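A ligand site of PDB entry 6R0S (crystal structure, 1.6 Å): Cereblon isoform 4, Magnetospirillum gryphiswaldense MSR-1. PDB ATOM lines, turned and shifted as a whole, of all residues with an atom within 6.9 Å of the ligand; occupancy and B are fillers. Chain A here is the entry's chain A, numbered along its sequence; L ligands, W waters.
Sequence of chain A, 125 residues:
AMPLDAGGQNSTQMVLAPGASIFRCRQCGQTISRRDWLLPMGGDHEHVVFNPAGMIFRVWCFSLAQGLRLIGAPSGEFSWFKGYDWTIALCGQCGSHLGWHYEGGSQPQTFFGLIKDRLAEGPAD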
ATOM      1  N   VAL A  49      -6.141 -18.137  18.180  1.00  0.00           N
ATOM      2  CA  VAL A  49      -6.956 -18.715  17.109  1.00  0.00           C
ATOM      3  C   VAL A  49      -8.232 -17.931  16.909  1.00  0.00           C
ATOM      4  O   VAL A  49      -8.580 -17.148  17.776  1.00  0.00           O
ATOM      5  CB  VAL A  49      -7.322 -20.185  17.446  1.00  0.00           C
ATOM      6  CG1 VAL A  49      -6.051 -21.034  17.498  1.00  0.00           C
ATOM      7  CG2 VAL A  49      -8.080 -20.295  18.779  1.00  0.00           C
ATOM      8  N   PHE A  50      -8.902 -18.118  15.770  1.00  0.00           N
ATOM      9  CA  PHE A  50     -10.231 -17.558  15.609  1.00  0.00           C
ATOM     10  C   PHE A  50     -11.216 -18.542  15.022  1.00  0.00           C
ATOM     11  O   PHE A  50     -10.822 -19.424  14.258  1.00  0.00           O
ATOM     12  CB  PHE A  50     -10.193 -16.235  14.832  1.00  0.00           C
ATOM     13  CG  PHE A  50      -9.869 -16.371  13.410  1.00  0.00           C
ATOM     14  CD1 PHE A  50     -10.884 -16.600  12.468  1.00  0.00           C
ATOM     15  CD2 PHE A  50      -8.582 -16.217  12.951  1.00  0.00           C
ATOM     16  CE1 PHE A  50     -10.618 -16.723  11.119  1.00  0.00           C
ATOM     17  CE2 PHE A  50      -8.294 -16.321  11.590  1.00  0.00           C
ATOM     18  CZ  PHE A  50      -9.333 -16.557  10.667  1.00  0.00           C
ATOM     19  N   ASN A  51     -12.483 -18.436  15.422  1.00  0.00           N
ATOM     20  CA  ASN A  51     -13.530 -19.317  14.907  1.00  0.00           C
ATOM     21  C   ASN A  51     -14.254 -18.715  13.667  1.00  0.00           C
ATOM     22  O   ASN A  51     -13.958 -17.592  13.248  1.00  0.00           O
ATOM     23  CB  ASN A  51     -14.490 -19.705  16.060  1.00  0.00           C
ATOM     24  CG  ASN A  51     -15.369 -18.558  16.543  1.00  0.00           C
ATOM     25  OD1 ASN A  51     -15.456 -17.489  15.920  1.00  0.00           O
ATOM     26  ND2 ASN A  51     -16.061 -18.786  17.613  1.00  0.00           N
ATOM     27  N   PRO A  52     -15.205 -19.452  13.077  1.00  0.00           N
ATOM     28  CA  PRO A  52     -15.890 -18.918  11.899  1.00  0.00           C
ATOM     29  C   PRO A  52     -16.691 -17.645  12.144  1.00  0.00           C
ATOM     30  O   PRO A  52     -16.940 -16.882  11.201  1.00  0.00           O
ATOM     31  CB  PRO A  52     -16.802 -20.056  11.462  1.00  0.00           C
ATOM     32  CG  PRO A  52     -16.086 -21.280  11.947  1.00  0.00           C
ATOM     33  CD  PRO A  52     -15.521 -20.887  13.281  1.00  0.00           C
ATOM     34  N   ALA A  53     -17.092 -17.421  13.396  1.00  0.00           N
ATOM     35  CA  ALA A  53     -17.786 -16.214  13.795  1.00  0.00           C
ATOM     36  C   ALA A  53     -16.836 -15.040  14.036  1.00  0.00           C
ATOM     37  O   ALA A  53     -17.280 -13.975  14.458  1.00  0.00           O
ATOM     38  CB  ALA A  53     -18.631 -16.491  15.014  1.00  0.00           C
ATOM     39  N   MET A  55     -14.477 -14.738  16.301  1.00  0.00           N
ATOM     40  CA  MET A  55     -14.061 -14.545  17.687  1.00  0.00           C
ATOM     41  C   MET A  55     -12.638 -15.053  17.819  1.00  0.00           C
ATOM     42  O   MET A  55     -12.326 -16.164  17.388  1.00  0.00           O
ATOM     43  CB  MET A  55     -14.970 -15.304  18.654  1.00  0.00           C
ATOM     44  CG  MET A  55     -14.615 -15.108  20.128  1.00  0.00           C
ATOM     45  SD  MET A  55     -14.457 -13.403  20.673  1.00  0.00           S
ATOM     46  CE  MET A  55     -16.073 -12.768  20.219  1.00  0.00           C
ATOM     47  N   PHE A  57      -9.570 -16.242  20.279  1.00  0.00           N
ATOM     48  CA  PHE A  57      -9.381 -16.884  21.569  1.00  0.00           C
ATOM     49  C   PHE A  57      -7.908 -17.092  21.773  1.00  0.00           C
ATOM     50  O   PHE A  57      -7.175 -17.475  20.848  1.00  0.00           O
ATOM     51  CB  PHE A  57     -10.051 -18.232  21.651  1.00  0.00           C
ATOM     52  CG  PHE A  57     -11.533 -18.227  21.351  1.00  0.00           C
ATOM     53  CD1 PHE A  57     -12.458 -17.982  22.346  1.00  0.00           C
ATOM     54  CD2 PHE A  57     -12.003 -18.520  20.079  1.00  0.00           C
ATOM     55  CE1 PHE A  57     -13.825 -18.021  22.093  1.00  0.00           C
ATOM     56  CE2 PHE A  57     -13.377 -18.518  19.822  1.00  0.00           C
ATOM     57  CZ  PHE A  57     -14.288 -18.299  20.824  1.00  0.00           C
ATOM     58  N   SER A  75     -16.467 -33.211  16.396  1.00  0.00           N
ATOM     59  CA  SER A  75     -16.422 -32.738  15.022  1.00  0.00           C
ATOM     60  C   SER A  75     -15.025 -32.350  14.626  1.00  0.00           C
ATOM     61  O   SER A  75     -14.289 -31.778  15.442  1.00  0.00           O
ATOM     62  CB  SER A  75     -17.316 -31.518  14.859  1.00  0.00           C
ATOM     63  OG  SER A  75     -17.228 -30.961  13.542  1.00  0.00           O
ATOM     64  N   GLY A  76     -14.616 -32.655  13.402  1.00  0.00           N
ATOM     65  CA  GLY A  76     -13.335 -32.190  12.870  1.00  0.00           C
ATOM     66  C   GLY A  76     -13.378 -30.853  12.170  1.00  0.00           C
ATOM     67  O   GLY A  76     -12.330 -30.315  11.834  1.00  0.00           O
ATOM     68  N   GLU A  77     -14.572 -30.308  11.954  1.00  0.00           N
ATOM     69  CA  GLU A  77     -14.777 -29.051  11.220  1.00  0.00           C
ATOM     70  C   GLU A  77     -14.019 -27.898  11.879  1.00  0.00           C
ATOM     71  O   GLU A  77     -14.199 -27.641  13.050  1.00  0.00           O
ATOM     72  CB  GLU A  77     -16.244 -28.661  11.207  1.00  0.00           C
ATOM     73  CG  GLU A  77     -17.162 -29.553  10.407  1.00  0.00           C
ATOM     74  CD  GLU A  77     -18.262 -28.725   9.739  1.00  0.00           C
ATOM     75  OE1 GLU A  77     -18.536 -27.582  10.216  1.00  0.00           O
ATOM     76  OE2 GLU A  77     -18.843 -29.176   8.735  1.00  0.00           O
ATOM     77  N   PHE A  78     -13.200 -27.228  11.095  1.00  0.00           N
ATOM     78  CA  PHE A  78     -12.491 -26.004  11.509  1.00  0.00           C
ATOM     79  C   PHE A  78     -11.528 -26.247  12.683  1.00  0.00           C
ATOM     80  O   PHE A  78     -11.138 -25.299  13.322  1.00  0.00           O
ATOM     81  CB  PHE A  78     -13.451 -24.870  11.883  1.00  0.00           C
ATOM     82  CG  PHE A  78     -14.556 -24.635  10.906  1.00  0.00           C
ATOM     83  CD1 PHE A  78     -14.305 -24.139   9.653  1.00  0.00           C
ATOM     84  CD2 PHE A  78     -15.866 -24.908  11.262  1.00  0.00           C
ATOM     85  CE1 PHE A  78     -15.345 -23.869   8.769  1.00  0.00           C
ATOM     86  CE2 PHE A  78     -16.915 -24.663  10.388  1.00  0.00           C
ATOM     87  CZ  PHE A  78     -16.655 -24.148   9.149  1.00  0.00           C
ATOM     88  N   SER A  79     -11.130 -27.473  12.952  1.00  0.00           N
ATOM     89  CA  SER A  79     -10.261 -27.734  14.065  1.00  0.00           C
ATOM     90  C   SER A  79      -8.949 -26.982  13.942  1.00  0.00           C
ATOM     91  O   SER A  79      -8.274 -27.002  12.925  1.00  0.00           O
ATOM     92  CB  SER A  79      -9.942 -29.211  14.238  1.00  0.00           C
ATOM     93  OG  SER A  79      -9.132 -29.391  15.377  1.00  0.00           O
ATOM     94  N   TRP A  80      -8.585 -26.318  15.031  1.00  0.00           N
ATOM     95  CA  TRP A  80      -7.347 -25.577  15.134  1.00  0.00           C
ATOM     96  C   TRP A  80      -6.143 -26.490  15.334  1.00  0.00           C
ATOM     97  O   TRP A  80      -5.011 -25.998  15.270  1.00  0.00           O
ATOM     98  CB  TRP A  80      -7.440 -24.595  16.299  1.00  0.00           C
ATOM     99  CG  TRP A  80      -8.482 -23.560  16.117  1.00  0.00           C
ATOM    100  CD1 TRP A  80      -8.703 -22.758  15.012  1.00  0.00           C
ATOM    101  CD2 TRP A  80      -9.431 -23.157  17.101  1.00  0.00           C
ATOM    102  NE1 TRP A  80      -9.752 -21.897  15.268  1.00  0.00           N
ATOM    103  CE2 TRP A  80     -10.194 -22.101  16.549  1.00  0.00           C
ATOM    104  CE3 TRP A  80      -9.700 -23.552  18.417  1.00  0.00           C
ATOM    105  CZ2 TRP A  80     -11.208 -21.485  17.249  1.00  0.00           C
ATOM    106  CZ3 TRP A  80     -10.714 -22.951  19.101  1.00  0.00           C
ATOM    107  CH2 TRP A  80     -11.452 -21.925  18.522  1.00  0.00           C
ATOM    108  N   PHE A  81      -6.355 -27.779  15.580  1.00  0.00           N
ATOM    109  CA  PHE A  81      -5.269 -28.701  15.884  1.00  0.00           C
ATOM    110  C   PHE A  81      -5.396 -29.883  14.951  1.00  0.00           C
ATOM    111  O   PHE A  81      -6.368 -30.650  15.019  1.00  0.00           O
ATOM    112  CB  PHE A  81      -5.301 -29.119  17.355  1.00  0.00           C
ATOM    113  CG  PHE A  81      -5.183 -27.962  18.299  1.00  0.00           C
ATOM    114  CD1 PHE A  81      -3.928 -27.454  18.618  1.00  0.00           C
ATOM    115  CD2 PHE A  81      -6.283 -27.405  18.855  1.00  0.00           C
ATOM    116  CE1 PHE A  81      -3.790 -26.447  19.571  1.00  0.00           C
ATOM    117  CE2 PHE A  81      -6.181 -26.320  19.732  1.00  0.00           C
ATOM    118  CZ  PHE A  81      -4.908 -25.855  20.117  1.00  0.00           C
ATOM    119  N   TYR A  84      -7.196 -33.599  15.203  1.00  0.00           N
ATOM    120  CA  TYR A  84      -8.090 -33.676  16.356  1.00  0.00           C
ATOM    121  C   TYR A  84      -9.495 -33.204  16.016  1.00  0.00           C
ATOM    122  O   TYR A  84      -9.685 -32.277  15.229  1.00  0.00           O
ATOM    123  CB  TYR A  84      -7.575 -32.827  17.507  1.00  0.00           C
ATOM    124  CG  TYR A  84      -6.283 -33.274  18.068  1.00  0.00           C
ATOM    125  CD1 TYR A  84      -6.209 -34.209  19.090  1.00  0.00           C
ATOM    126  CD2 TYR A  84      -5.101 -32.724  17.613  1.00  0.00           C
ATOM    127  CE1 TYR A  84      -4.987 -34.596  19.622  1.00  0.00           C
ATOM    128  CE2 TYR A  84      -3.864 -33.107  18.129  1.00  0.00           C
ATOM    129  CZ  TYR A  84      -3.818 -34.085  19.086  1.00  0.00           C
ATOM    130  OH  TYR A  84      -2.623 -34.442  19.611  1.00  0.00           O
ATOM    131  N   TRP A  86     -13.148 -32.019  17.918  1.00  0.00           N
ATOM    132  CA  TRP A  86     -13.467 -31.241  19.140  1.00  0.00           C
ATOM    133  C   TRP A  86     -14.899 -31.412  19.593  1.00  0.00           C
ATOM    134  O   TRP A  86     -15.820 -31.681  18.799  1.00  0.00           O
ATOM    135  CB  TRP A  86     -13.149 -29.763  18.964  1.00  0.00           C
ATOM    136  CG  TRP A  86     -13.788 -29.166  17.763  1.00  0.00           C
ATOM    137  CD1 TRP A  86     -13.232 -29.027  16.537  1.00  0.00           C
ATOM    138  CD2 TRP A  86     -15.131 -28.654  17.667  1.00  0.00           C
ATOM    139  NE1 TRP A  86     -14.134 -28.461  15.675  1.00  0.00           N
ATOM    140  CE2 TRP A  86     -15.316 -28.252  16.335  1.00  0.00           C
ATOM    141  CE3 TRP A  86     -16.194 -28.516  18.568  1.00  0.00           C
ATOM    142  CZ2 TRP A  86     -16.524 -27.722  15.878  1.00  0.00           C
ATOM    143  CZ3 TRP A  86     -17.394 -27.967  18.124  1.00  0.00           C
ATOM    144  CH2 TRP A  86     -17.539 -27.580  16.789  1.00  0.00           C
ATOM    145  N   THR A  87     -15.084 -31.191  20.898  1.00  0.00           N
ATOM    146  CA  THR A  87     -16.394 -31.093  21.518  1.00  0.00           C
ATOM    147  C   THR A  87     -16.342 -29.861  22.394  1.00  0.00           C
ATOM    148  O   THR A  87     -15.318 -29.548  22.987  1.00  0.00           O
ATOM    149  CB  THR A  87     -16.745 -32.304  22.407  1.00  0.00           C
ATOM    150  OG1 THR A  87     -15.734 -32.564  23.381  1.00  0.00           O
ATOM    151  CG2 THR A  87     -17.057 -33.546  21.557  1.00  0.00           C
ATOM    152  N   ILE A  88     -17.455 -29.148  22.436  1.00  0.00           N
ATOM    153  CA  ILE A  88     -17.548 -27.953  23.280  1.00  0.00           C
ATOM    154  C   ILE A  88     -17.486 -28.397  24.730  1.00  0.00           C
ATOM    155  O   ILE A  88     -18.132 -29.404  25.136  1.00  0.00           O
ATOM    156  CB  ILE A  88     -18.857 -27.199  22.988  1.00  0.00           C
ATOM    157  CG1 ILE A  88     -18.745 -26.530  21.613  1.00  0.00           C
ATOM    158  CG2 ILE A  88     -19.198 -26.179  24.081  1.00  0.00           C
ATOM    159  CD1 ILE A  88     -20.058 -26.004  21.082  1.00  0.00           C
ATOM    160  N   HIS A  97     -19.006 -21.246  28.707  1.00  0.00           N
ATOM    161  CA  HIS A  97     -18.217 -21.944  27.704  1.00  0.00           C
ATOM    162  C   HIS A  97     -16.741 -21.721  27.963  1.00  0.00           C
ATOM    163  O   HIS A  97     -16.239 -20.613  27.778  1.00  0.00           O
ATOM    164  CB  HIS A  97     -18.598 -21.450  26.313  1.00  0.00           C
ATOM    165  CG  HIS A  97     -17.799 -22.091  25.244  1.00  0.00           C
ATOM    166  ND1 HIS A  97     -17.583 -21.476  24.030  1.00  0.00           N
ATOM    167  CD2 HIS A  97     -17.137 -23.272  25.222  1.00  0.00           C
ATOM    168  CE1 HIS A  97     -16.827 -22.268  23.298  1.00  0.00           C
ATOM    169  NE2 HIS A  97     -16.539 -23.356  23.984  1.00  0.00           N
ATOM    170  N   TRP A 100     -12.764 -26.340  24.695  1.00  0.00           N
ATOM    171  CA  TRP A 100     -13.066 -27.529  23.899  1.00  0.00           C
ATOM    172  C   TRP A 100     -12.226 -28.689  24.387  1.00  0.00           C
ATOM    173  O   TRP A 100     -11.110 -28.492  24.884  1.00  0.00           O
ATOM    174  CB  TRP A 100     -12.770 -27.269  22.410  1.00  0.00           C
ATOM    175  CG  TRP A 100     -13.501 -26.088  21.837  1.00  0.00           C
ATOM    176  CD1 TRP A 100     -14.707 -26.099  21.212  1.00  0.00           C
ATOM    177  CD2 TRP A 100     -13.124 -24.703  21.933  1.00  0.00           C
ATOM    178  NE1 TRP A 100     -15.096 -24.822  20.901  1.00  0.00           N
ATOM    179  CE2 TRP A 100     -14.133 -23.942  21.314  1.00  0.00           C
ATOM    180  CE3 TRP A 100     -12.014 -24.037  22.473  1.00  0.00           C
ATOM    181  CZ2 TRP A 100     -14.079 -22.555  21.216  1.00  0.00           C
ATOM    182  CZ3 TRP A 100     -11.978 -22.642  22.398  1.00  0.00           C
ATOM    183  CH2 TRP A 100     -13.006 -21.933  21.792  1.00  0.00           C
ATOM    184  N   TYR A 102     -10.429 -32.034  22.872  1.00  0.00           N
ATOM    185  CA  TYR A 102      -9.922 -32.548  21.587  1.00  0.00           C
ATOM    186  C   TYR A 102      -9.644 -34.034  21.761  1.00  0.00           C
ATOM    187  O   TYR A 102      -9.140 -34.459  22.785  1.00  0.00           O
ATOM    188  CB  TYR A 102      -8.654 -31.786  21.197  1.00  0.00           C
ATOM    189  CG  TYR A 102      -8.964 -30.382  20.778  1.00  0.00           C
ATOM    190  CD1 TYR A 102      -9.362 -30.105  19.472  1.00  0.00           C
ATOM    191  CD2 TYR A 102      -8.944 -29.339  21.699  1.00  0.00           C
ATOM    192  CE1 TYR A 102      -9.680 -28.789  19.088  1.00  0.00           C
ATOM    193  CE2 TYR A 102      -9.251 -28.037  21.328  1.00  0.00           C
ATOM    194  CZ  TYR A 102      -9.629 -27.786  20.017  1.00  0.00           C
ATOM    195  OH  TYR A 102      -9.946 -26.501  19.600  1.00  0.00           O
HETATM  196  O1  LIG L   1     -13.445 -22.922  15.037  1.00  0.00           O
HETATM  197  C1  LIG L   1     -13.265 -23.787  15.988  1.00  0.00           C
HETATM  198  N1  LIG L   1     -12.184 -24.600  15.936  1.00  0.00           N
HETATM  199  C2  LIG L   1     -11.949 -25.488  16.951  1.00  0.00           C
HETATM  200  O2  LIG L   1     -10.953 -26.144  16.999  1.00  0.00           O
HETATM  201  C3  LIG L   1     -12.974 -25.602  18.047  1.00  0.00           C
HETATM  202  C4  LIG L   1     -14.372 -25.250  17.588  1.00  0.00           C
HETATM  203  C5  LIG L   1     -14.298 -23.843  17.098  1.00  0.00           C
HETATM  204  N2  LIG L   1     -15.620 -23.363  16.585  1.00  0.00           N
HETATM  205  C6  LIG L   1     -19.675 -22.093  14.673  1.00  0.00           C
HETATM  206  C7  LIG L   1     -18.638 -23.018  14.498  1.00  0.00           C
HETATM  207  C8  LIG L   1     -17.571 -23.004  15.401  1.00  0.00           C
HETATM  208  C9  LIG L   1     -17.532 -22.087  16.420  1.00  0.00           C
HETATM  209  O3  LIG L   1     -15.928 -24.776  14.710  1.00  0.00           O
HETATM  210  O4  LIG L   1     -15.822 -21.714  18.207  1.00  0.00           O
HETATM  211  C10 LIG L   1     -18.553 -21.165  16.636  1.00  0.00           C
HETATM  212  C11 LIG L   1     -19.628 -21.161  15.728  1.00  0.00           C
HETATM  213  C12 LIG L   1     -16.353 -22.392  17.082  1.00  0.00           C
HETATM  214  C13 LIG L   1     -16.391 -23.712  15.550  1.00  0.00           C
HETATM  215  O   HOH W   1     -17.922 -21.343  20.099  1.00  0.00           O
HETATM  216  O   HOH W   2     -18.436 -26.314  13.453  1.00  0.00           O
HETATM  217  O   HOH W   3     -17.532 -24.153  19.429  1.00  0.00           O
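A nitrogen (N1) of the ligand sits at hydrogen-bond distance from the backbone carbonyl oxygen of Phe 78 (2.9 Å).
The side-chain hydroxyl (OH) of Tyr 102 lies within hydrogen-bond range of an oxygen (O2) of the ligand, 2.8 Å away.
The side-chain amide nitrogen (ND2) of Asn 51 sits at hydrogen-bond distance from an oxygen (O4) of the ligand (3.0 Å).
O2 of the ligand sits at hydrogen-bond distance from N of Trp 80 (3.1 Å).
OD1 of Asn 51 is in hydrogen-bond range of N of Ala 53 (3.0 Å).
The side-chain hydroxyl of Ser 75 is in hydrogen-bond range of the backbone NH of Glu 77, 3.2 Å away.
The backbone NH (N) of Trp 86 is in hydrogen-bond range of the backbone carbonyl oxygen (O) of Ser 75 (2.7 Å).
O of Phe 81 lies within hydrogen-bond range of OG of Ser 79, at 3.1 Å.
The backbone NH (N) of Met 55 lies within hydrogen-bond range of the side-chain amide oxygen (OD1) of Asn 51.
OG of Ser 79 sits at hydrogen-bond distance from O of Tyr 84 (2.9 Å).
The indole nitrogen (NE1) of Trp 80 lies within hydrogen-bond range of the backbone carbonyl oxygen (O) of Phe 50 (2.9 Å).
The indole nitrogen (NE1) of Trp 86 lies within hydrogen-bond range of the backbone carbonyl oxygen (O) of Glu 77 (2.8 Å).
Pro 52 touches the ligand (CD to O1, 3.4 Å).
O of Glu 77 touches O3 of the ligand, 3.7 Å away.
CA of Ser 79 touches O2 of the ligand, 3.4 Å away.
Trp 86 touches the ligand.
NE1 of Trp 100 touches C4 of the ligand, at 3.4 Å.
Of the 21 residues printed, 9 come within 4 Å of the ligand.
Water W3 lies within hydrogen-bond range of NE1 of Trp 100 (2.9 Å) and O4 of the ligand (3.2 Å).
Water W2 bridges an oxygen (O3) of the ligand (3.2 Å) and the side-chain carboxylate (OE1) of Glu 77 (3.5 Å).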
